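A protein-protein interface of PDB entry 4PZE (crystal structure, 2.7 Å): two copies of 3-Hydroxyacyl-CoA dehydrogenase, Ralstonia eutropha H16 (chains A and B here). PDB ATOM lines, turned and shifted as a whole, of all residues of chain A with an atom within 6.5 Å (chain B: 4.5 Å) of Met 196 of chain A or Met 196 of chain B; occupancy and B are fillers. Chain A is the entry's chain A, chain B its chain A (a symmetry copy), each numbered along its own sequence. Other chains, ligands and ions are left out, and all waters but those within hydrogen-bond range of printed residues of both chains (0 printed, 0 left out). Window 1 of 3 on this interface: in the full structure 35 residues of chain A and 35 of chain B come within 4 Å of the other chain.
SD of Met 196 of chain A sits close to SD of Met 196 of chain B. The guanidinium group of Arg 191 of chain A lies within salt-bridge range of the side-chain carboxylate of Glu 199 of chain B, at 2.8 Å.
Among the printed residues, pairs that only touch across the chains: Ile 192 of chain A with Met 196 of chain B (3.6 Å), Ile 192 of chain A with Glu 199 of chain B (3.3 Å), Ile 192 of chain A with Ala 200 of chain B (3.5 Å), Met 196 of chain A with Ile 192 of chain B (3.6 Å), Glu 199 of chain A with Ile 192 of chain B (3.3 Å), Ala 200 of chain A with Ile 192 of chain B (3.5 Å) and Met 218 of chain A with Ile 192 of chain B (3.2 Å).
Printed residues of chain B within 4 Å of Arg 191 of chain A: Glu 199. Of the printed residues of chain B, Ile 192 of chain A touches Met 196 (3.6 Å), Glu 199 (3.3 Å) and Ala 200 (3.5 Å). Of chain B, only Ile 192 (3.6 Å) and Met 196 (3.6 Å) come within 4 Å of Met 196 of chain A. Of the printed residues of chain A, Ile 192 of chain B touches Met 196, Glu 199, Ala 200 and Met 218. Cys 194 of chain B touches none of the printed residues of chain A. Pro 195 of chain B touches none of the printed residues of chain A. Met 196 of chain B touches just these residues of chain A: Ile 192 (3.6 Å) and Met 196 (3.6 Å). Of the printed residues of chain A, Glu 199 of chain B touches Arg 191 (2.8 Å) and Ile 192 (3.3 Å). The nearest printed residue of chain B that does not touch Met 196 of chain A is Leu 193 of chain B (5.1 Å). The nearest residue of chain A that does not touch Met 196 of chain B is Leu 193 of chain A (5.1 Å). The nearest printed residue of chain B that does not touch Glu 199 of chain A is Pro 195 of chain B (5.0 Å).
Of the 10 printed residues of chain B, 4 touch a printed residue of chain A. Hydrophobic or aromatic side chains of chain A within 4 Å of the printed part of chain B: Ile 192, Met 196 and Met 218.
Ile 192 of chain A touches Met 196 of chain B, and with the chains exchanged Met 196 of chain A touches Ile 192 of chain B. Ile 192 of chain A touches Glu 199 of chain B, and with the chains exchanged Glu 199 of chain A touches Ile 192 of chain B. Ile 192 of chain A touches Ala 200 of chain B, and with the chains exchanged Ala 200 of chain A touches Ile 192 of chain B. Met 196 of chain A touches its own counterpart, Met 196 of chain B. Positions printed for both chains: 192, 193, 194, 195, 196, 197, 198, 199, 200 and 228.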
ATOM      1  N   ARG A 191      -1.514   0.405  33.965  1.00  0.00           N
ATOM      2  CA  ARG A 191      -1.351  -0.475  32.812  1.00  0.00           C
ATOM      3  C   ARG A 191      -1.199   0.277  31.529  1.00  0.00           C
ATOM      4  O   ARG A 191      -0.289  -0.031  30.754  1.00  0.00           O
ATOM      5  CB  ARG A 191      -2.476  -1.475  32.694  1.00  0.00           C
ATOM      6  CG  ARG A 191      -2.039  -2.748  31.968  1.00  0.00           C
ATOM      7  CD  ARG A 191      -2.276  -2.584  30.515  1.00  0.00           C
ATOM      8  NE  ARG A 191      -1.984  -3.719  29.652  1.00  0.00           N
ATOM      9  CZ  ARG A 191      -2.666  -4.860  29.591  1.00  0.00           C
ATOM     10  NH1 ARG A 191      -3.643  -5.169  30.452  1.00  0.00           N
ATOM     11  NH2 ARG A 191      -2.320  -5.729  28.663  1.00  0.00           N
ATOM     12  N   ILE A 192      -2.064   1.254  31.293  1.00  0.00           N
ATOM     13  CA  ILE A 192      -1.874   2.095  30.116  1.00  0.00           C
ATOM     14  C   ILE A 192      -0.988   3.337  30.303  1.00  0.00           C
ATOM     15  O   ILE A 192      -0.273   3.706  29.379  1.00  0.00           O
ATOM     16  CB  ILE A 192      -3.203   2.378  29.358  1.00  0.00           C
ATOM     17  CG1 ILE A 192      -4.259   3.081  30.195  1.00  0.00           C
ATOM     18  CG2 ILE A 192      -3.774   1.057  28.880  1.00  0.00           C
ATOM     19  CD1 ILE A 192      -5.645   2.407  30.169  1.00  0.00           C
ATOM     20  N   LEU A 193      -0.987   3.970  31.477  1.00  0.00           N
ATOM     21  CA  LEU A 193      -0.167   5.171  31.661  1.00  0.00           C
ATOM     22  C   LEU A 193       1.318   4.821  31.597  1.00  0.00           C
ATOM     23  O   LEU A 193       2.073   5.410  30.838  1.00  0.00           O
ATOM     24  CB  LEU A 193      -0.500   5.901  32.975  1.00  0.00           C
ATOM     25  CG  LEU A 193       0.362   7.151  33.375  1.00  0.00           C
ATOM     26  CD1 LEU A 193      -0.038   8.416  32.621  1.00  0.00           C
ATOM     27  CD2 LEU A 193       0.370   7.447  34.880  1.00  0.00           C
ATOM     28  N   CYS A 194       1.751   3.838  32.365  1.00  0.00           N
ATOM     29  CA  CYS A 194       3.197   3.668  32.541  1.00  0.00           C
ATOM     30  C   CYS A 194       3.952   3.265  31.293  1.00  0.00           C
ATOM     31  O   CYS A 194       5.042   3.766  31.077  1.00  0.00           O
ATOM     32  CB  CYS A 194       3.519   2.758  33.720  1.00  0.00           C
ATOM     33  SG  CYS A 194       3.034   3.444  35.338  1.00  0.00           S
ATOM     34  N   PRO A 195       3.374   2.389  30.444  1.00  0.00           N
ATOM     35  CA  PRO A 195       4.110   2.046  29.214  1.00  0.00           C
ATOM     36  C   PRO A 195       4.246   3.210  28.244  1.00  0.00           C
ATOM     37  O   PRO A 195       5.131   3.205  27.378  1.00  0.00           O
ATOM     38  CB  PRO A 195       3.286   0.922  28.614  1.00  0.00           C
ATOM     39  CG  PRO A 195       2.605   0.314  29.785  1.00  0.00           C
ATOM     40  CD  PRO A 195       2.235   1.484  30.637  1.00  0.00           C
ATOM     41  N   MET A 196       3.397   4.213  28.419  1.00  0.00           N
ATOM     42  CA  MET A 196       3.535   5.450  27.689  1.00  0.00           C
ATOM     43  C   MET A 196       4.719   6.234  28.225  1.00  0.00           C
ATOM     44  O   MET A 196       5.510   6.738  27.431  1.00  0.00           O
ATOM     45  CB  MET A 196       2.278   6.295  27.822  1.00  0.00           C
ATOM     46  CG  MET A 196       2.224   7.457  26.855  1.00  0.00           C
ATOM     47  SD  MET A 196       1.152   8.713  27.528  1.00  0.00           S
ATOM     48  CE  MET A 196       2.356   9.558  28.548  1.00  0.00           C
ATOM     49  N   ILE A 197       4.848   6.350  29.552  1.00  0.00           N
ATOM     50  CA  ILE A 197       5.985   7.082  30.094  1.00  0.00           C
ATOM     51  C   ILE A 197       7.245   6.406  29.498  1.00  0.00           C
ATOM     52  O   ILE A 197       8.104   7.037  28.870  1.00  0.00           O
ATOM     53  CB  ILE A 197       6.076   7.077  31.646  1.00  0.00           C
ATOM     54  CG1 ILE A 197       4.735   7.339  32.371  1.00  0.00           C
ATOM     55  CG2 ILE A 197       7.078   8.127  32.100  1.00  0.00           C
ATOM     56  CD1 ILE A 197       4.186   8.733  32.193  1.00  0.00           C
ATOM     57  N   ASN A 198       7.294   5.093  29.632  1.00  0.00           N
ATOM     58  CA  ASN A 198       8.345   4.307  29.025  1.00  0.00           C
ATOM     59  C   ASN A 198       8.647   4.611  27.548  1.00  0.00           C
ATOM     60  O   ASN A 198       9.803   4.654  27.115  1.00  0.00           O
ATOM     61  CB  ASN A 198       8.007   2.841  29.166  1.00  0.00           C
ATOM     62  CG  ASN A 198       9.232   1.987  29.225  1.00  0.00           C
ATOM     63  OD1 ASN A 198       9.490   1.173  28.351  1.00  0.00           O
ATOM     64  ND2 ASN A 198      10.002   2.171  30.272  1.00  0.00           N
ATOM     65  N   GLU A 199       7.612   4.812  26.758  1.00  0.00           N
ATOM     66  CA  GLU A 199       7.835   5.113  25.373  1.00  0.00           C
ATOM     67  C   GLU A 199       8.505   6.473  25.170  1.00  0.00           C
ATOM     68  O   GLU A 199       9.206   6.662  24.171  1.00  0.00           O
ATOM     69  CB  GLU A 199       6.518   5.032  24.612  1.00  0.00           C
ATOM     70  CG  GLU A 199       6.701   4.740  23.123  1.00  0.00           C
ATOM     71  CD  GLU A 199       7.257   3.354  22.869  1.00  0.00           C
ATOM     72  OE1 GLU A 199       7.113   2.494  23.781  1.00  0.00           O
ATOM     73  OE2 GLU A 199       7.846   3.160  21.770  1.00  0.00           O
ATOM     74  N   ALA A 200       8.262   7.431  26.081  1.00  0.00           N
ATOM     75  CA  ALA A 200       8.979   8.724  26.086  1.00  0.00           C
ATOM     76  C   ALA A 200      10.453   8.510  26.350  1.00  0.00           C
ATOM     77  O   ALA A 200      11.283   9.010  25.617  1.00  0.00           O
ATOM     78  CB  ALA A 200       8.410   9.672  27.120  1.00  0.00           C
ATOM     79  N   PHE A 201      10.791   7.722  27.362  1.00  0.00           N
ATOM     80  CA  PHE A 201      12.197   7.359  27.579  1.00  0.00           C
ATOM     81  C   PHE A 201      12.822   6.668  26.353  1.00  0.00           C
ATOM     82  O   PHE A 201      13.995   6.934  26.027  1.00  0.00           O
ATOM     83  CB  PHE A 201      12.372   6.527  28.869  1.00  0.00           C
ATOM     84  CG  PHE A 201      12.238   7.353  30.136  1.00  0.00           C
ATOM     85  CD1 PHE A 201      10.993   7.747  30.604  1.00  0.00           C
ATOM     86  CD2 PHE A 201      13.360   7.778  30.835  1.00  0.00           C
ATOM     87  CE1 PHE A 201      10.866   8.522  31.740  1.00  0.00           C
ATOM     88  CE2 PHE A 201      13.240   8.558  31.975  1.00  0.00           C
ATOM     89  CZ  PHE A 201      11.989   8.928  32.429  1.00  0.00           C
ATOM     90  N   MET A 218       3.665  16.632  23.945  1.00  0.00           N
ATOM     91  CA  MET A 218       2.533  15.924  24.551  1.00  0.00           C
ATOM     92  C   MET A 218       1.579  16.874  25.286  1.00  0.00           C
ATOM     93  O   MET A 218       0.356  16.623  25.294  1.00  0.00           O
ATOM     94  CB  MET A 218       3.009  14.798  25.514  1.00  0.00           C
ATOM     95  CG  MET A 218       3.893  13.716  24.887  1.00  0.00           C
ATOM     96  SD  MET A 218       3.251  12.861  23.424  1.00  0.00           S
ATOM     97  CE  MET A 218       1.894  12.027  24.234  1.00  0.00           C
ATOM     98  N   HIS A 224      -2.146  17.445  27.600  1.00  0.00           N
ATOM     99  CA  HIS A 224      -1.833  16.822  28.872  1.00  0.00           C
ATOM    100  C   HIS A 224      -1.317  17.925  29.806  1.00  0.00           C
ATOM    101  O   HIS A 224      -0.570  18.786  29.365  1.00  0.00           O
ATOM    102  CB  HIS A 224      -0.769  15.733  28.725  1.00  0.00           C
ATOM    103  CG  HIS A 224      -1.254  14.479  28.065  1.00  0.00           C
ATOM    104  ND1 HIS A 224      -0.409  13.618  27.396  1.00  0.00           N
ATOM    105  CD2 HIS A 224      -2.489  13.945  27.954  1.00  0.00           C
ATOM    106  CE1 HIS A 224      -1.101  12.606  26.907  1.00  0.00           C
ATOM    107  NE2 HIS A 224      -2.368  12.783  27.231  1.00  0.00           N
ATOM    108  N   GLY A 227       4.079  16.820  30.939  1.00  0.00           N
ATOM    109  CA  GLY A 227       4.690  15.934  29.977  1.00  0.00           C
ATOM    110  C   GLY A 227       5.142  14.709  30.729  1.00  0.00           C
ATOM    111  O   GLY A 227       5.455  14.817  31.915  1.00  0.00           O
ATOM    112  N   PRO A 228       5.187  13.544  30.047  1.00  0.00           N
ATOM    113  CA  PRO A 228       5.510  12.278  30.704  1.00  0.00           C
ATOM    114  C   PRO A 228       6.889  12.264  31.387  1.00  0.00           C
ATOM    115  O   PRO A 228       7.035  11.676  32.469  1.00  0.00           O
ATOM    116  CB  PRO A 228       5.485  11.262  29.554  1.00  0.00           C
ATOM    117  CG  PRO A 228       5.824  12.047  28.333  1.00  0.00           C
ATOM    118  CD  PRO A 228       5.349  13.464  28.586  1.00  0.00           C
ATOM    119  N   LEU A 231       6.708  14.174  34.422  1.00  0.00           N
ATOM    120  CA  LEU A 231       5.870  13.337  35.224  1.00  0.00           C
ATOM    121  C   LEU A 231       6.655  12.175  35.802  1.00  0.00           C
ATOM    122  O   LEU A 231       6.437  11.776  36.951  1.00  0.00           O
ATOM    123  CB  LEU A 231       4.711  12.809  34.376  1.00  0.00           C
ATOM    124  CG  LEU A 231       3.633  12.113  35.224  1.00  0.00           C
ATOM    125  CD1 LEU A 231       3.109  13.083  36.275  1.00  0.00           C
ATOM    126  CD2 LEU A 231       2.494  11.533  34.389  1.00  0.00           C
ATOM    127  N   MET A 244       7.234  -1.087  35.220  1.00  0.00           N
ATOM    128  CA  MET A 244       7.638  -1.765  34.021  1.00  0.00           C
ATOM    129  C   MET A 244       8.244  -3.145  34.252  1.00  0.00           C
ATOM    130  O   MET A 244       8.081  -4.015  33.415  1.00  0.00           O
ATOM    131  CB  MET A 244       8.614  -0.921  33.213  1.00  0.00           C
ATOM    132  CG  MET A 244       8.065   0.376  32.628  1.00  0.00           C
ATOM    133  SD  MET A 244       6.550   0.287  31.672  1.00  0.00           S
ATOM    134  CE  MET A 244       5.504   0.146  33.091  1.00  0.00           C
ATOM    135  N   ILE B 192       4.439   8.165  20.946  1.00  0.00           N
ATOM    136  CA  ILE B 192       4.008   7.805  22.292  1.00  0.00           C
ATOM    137  C   ILE B 192       2.492   7.818  22.547  1.00  0.00           C
ATOM    138  O   ILE B 192       2.008   6.991  23.310  1.00  0.00           O
ATOM    139  CB  ILE B 192       4.839   8.514  23.400  1.00  0.00           C
ATOM    140  CG1 ILE B 192       4.781  10.031  23.346  1.00  0.00           C
ATOM    141  CG2 ILE B 192       6.287   8.086  23.261  1.00  0.00           C
ATOM    142  CD1 ILE B 192       6.158  10.724  23.379  1.00  0.00           C
ATOM    143  N   LEU B 193       1.728   8.706  21.910  1.00  0.00           N
ATOM    144  CA  LEU B 193       0.284   8.747  22.164  1.00  0.00           C
ATOM    145  C   LEU B 193      -0.385   7.473  21.655  1.00  0.00           C
ATOM    146  O   LEU B 193      -1.099   6.800  22.385  1.00  0.00           O
ATOM    147  CB  LEU B 193      -0.374   9.994  21.547  1.00  0.00           C
ATOM    148  CG  LEU B 193      -1.935  10.137  21.638  1.00  0.00           C
ATOM    149  CD1 LEU B 193      -2.410  10.616  23.007  1.00  0.00           C
ATOM    150  CD2 LEU B 193      -2.544  11.037  20.555  1.00  0.00           C
ATOM    151  N   CYS B 194      -0.141   7.104  20.410  1.00  0.00           N
ATOM    152  CA  CYS B 194      -0.979   6.063  19.807  1.00  0.00           C
ATOM    153  C   CYS B 194      -0.842   4.690  20.429  1.00  0.00           C
ATOM    154  O   CYS B 194      -1.844   4.012  20.583  1.00  0.00           O
ATOM    155  CB  CYS B 194      -0.822   6.020  18.292  1.00  0.00           C
ATOM    156  SG  CYS B 194      -1.431   7.515  17.443  1.00  0.00           S
ATOM    157  N   PRO B 195       0.380   4.280  20.824  1.00  0.00           N
ATOM    158  CA  PRO B 195       0.480   2.957  21.467  1.00  0.00           C
ATOM    159  C   PRO B 195      -0.205   2.888  22.823  1.00  0.00           C
ATOM    160  O   PRO B 195      -0.540   1.796  23.303  1.00  0.00           O
ATOM    161  CB  PRO B 195       1.977   2.741  21.595  1.00  0.00           C
ATOM    162  CG  PRO B 195       2.551   3.562  20.499  1.00  0.00           C
ATOM    163  CD  PRO B 195       1.713   4.799  20.495  1.00  0.00           C
ATOM    164  N   MET B 196      -0.443   4.052  23.412  1.00  0.00           N
ATOM    165  CA  MET B 196      -1.245   4.138  24.609  1.00  0.00           C
ATOM    166  C   MET B 196      -2.705   3.905  24.267  1.00  0.00           C
ATOM    167  O   MET B 196      -3.371   3.150  24.973  1.00  0.00           O
ATOM    168  CB  MET B 196      -1.098   5.506  25.257  1.00  0.00           C
ATOM    169  CG  MET B 196      -1.662   5.577  26.658  1.00  0.00           C
ATOM    170  SD  MET B 196      -2.072   7.272  27.026  1.00  0.00           S
ATOM    171  CE  MET B 196      -3.713   7.300  26.314  1.00  0.00           C
ATOM    172  N   ILE B 197      -3.213   4.544  23.207  1.00  0.00           N
ATOM    173  CA  ILE B 197      -4.607   4.324  22.844  1.00  0.00           C
ATOM    174  C   ILE B 197      -4.760   2.793  22.663  1.00  0.00           C
ATOM    175  O   ILE B 197      -5.604   2.131  23.280  1.00  0.00           O
ATOM    176  CB  ILE B 197      -5.061   5.051  21.548  1.00  0.00           C
ATOM    177  CG1 ILE B 197      -4.587   6.519  21.433  1.00  0.00           C
ATOM    178  CG2 ILE B 197      -6.579   5.029  21.456  1.00  0.00           C
ATOM    179  CD1 ILE B 197      -5.210   7.460  22.434  1.00  0.00           C
ATOM    180  N   ASN B 198      -3.868   2.231  21.868  1.00  0.00           N
ATOM    181  CA  ASN B 198      -3.805   0.797  21.691  1.00  0.00           C
ATOM    182  C   ASN B 198      -3.839  -0.042  22.980  1.00  0.00           C
ATOM    183  O   ASN B 198      -4.491  -1.088  23.060  1.00  0.00           O
ATOM    184  CB  ASN B 198      -2.558   0.451  20.912  1.00  0.00           C
ATOM    185  CG  ASN B 198      -2.728  -0.799  20.110  1.00  0.00           C
ATOM    186  OD1 ASN B 198      -2.072  -1.804  20.343  1.00  0.00           O
ATOM    187  ND2 ASN B 198      -3.619  -0.741  19.149  1.00  0.00           N
ATOM    188  N   GLU B 199      -3.125   0.398  23.996  1.00  0.00           N
ATOM    189  CA  GLU B 199      -3.130  -0.338  25.228  1.00  0.00           C
ATOM    190  C   GLU B 199      -4.495  -0.314  25.919  1.00  0.00           C
ATOM    191  O   GLU B 199      -4.820  -1.251  26.653  1.00  0.00           O
ATOM    192  CB  GLU B 199      -2.040   0.197  26.148  1.00  0.00           C
ATOM    193  CG  GLU B 199      -1.561  -0.833  27.172  1.00  0.00           C
ATOM    194  CD  GLU B 199      -0.837  -1.997  26.526  1.00  0.00           C
ATOM    195  OE1 GLU B 199      -0.354  -1.815  25.376  1.00  0.00           O
ATOM    196  OE2 GLU B 199      -0.787  -3.077  27.176  1.00  0.00           O
ATOM    197  N   ALA B 200      -5.273   0.766  25.726  1.00  0.00           N
ATOM    198  CA  ALA B 200      -6.672   0.831  26.201  1.00  0.00           C
ATOM    199  C   ALA B 200      -7.519  -0.206  25.495  1.00  0.00           C
ATOM    200  O   ALA B 200      -8.221  -0.960  26.139  1.00  0.00           O
ATOM    201  CB  ALA B 200      -7.268   2.206  25.986  1.00  0.00           C
ATOM    202  N   PRO B 228      -8.801   7.812  26.400  1.00  0.00           N
ATOM    203  CA  PRO B 228      -8.252   7.339  25.130  1.00  0.00           C
ATOM    204  C   PRO B 228      -9.292   6.677  24.209  1.00  0.00           C
ATOM    205  O   PRO B 228      -9.233   6.858  22.984  1.00  0.00           O
ATOM    206  CB  PRO B 228      -7.199   6.307  25.559  1.00  0.00           C
ATOM    207  CG  PRO B 228      -7.673   5.790  26.873  1.00  0.00           C
ATOM    208  CD  PRO B 228      -8.469   6.908  27.515  1.00  0.00           C
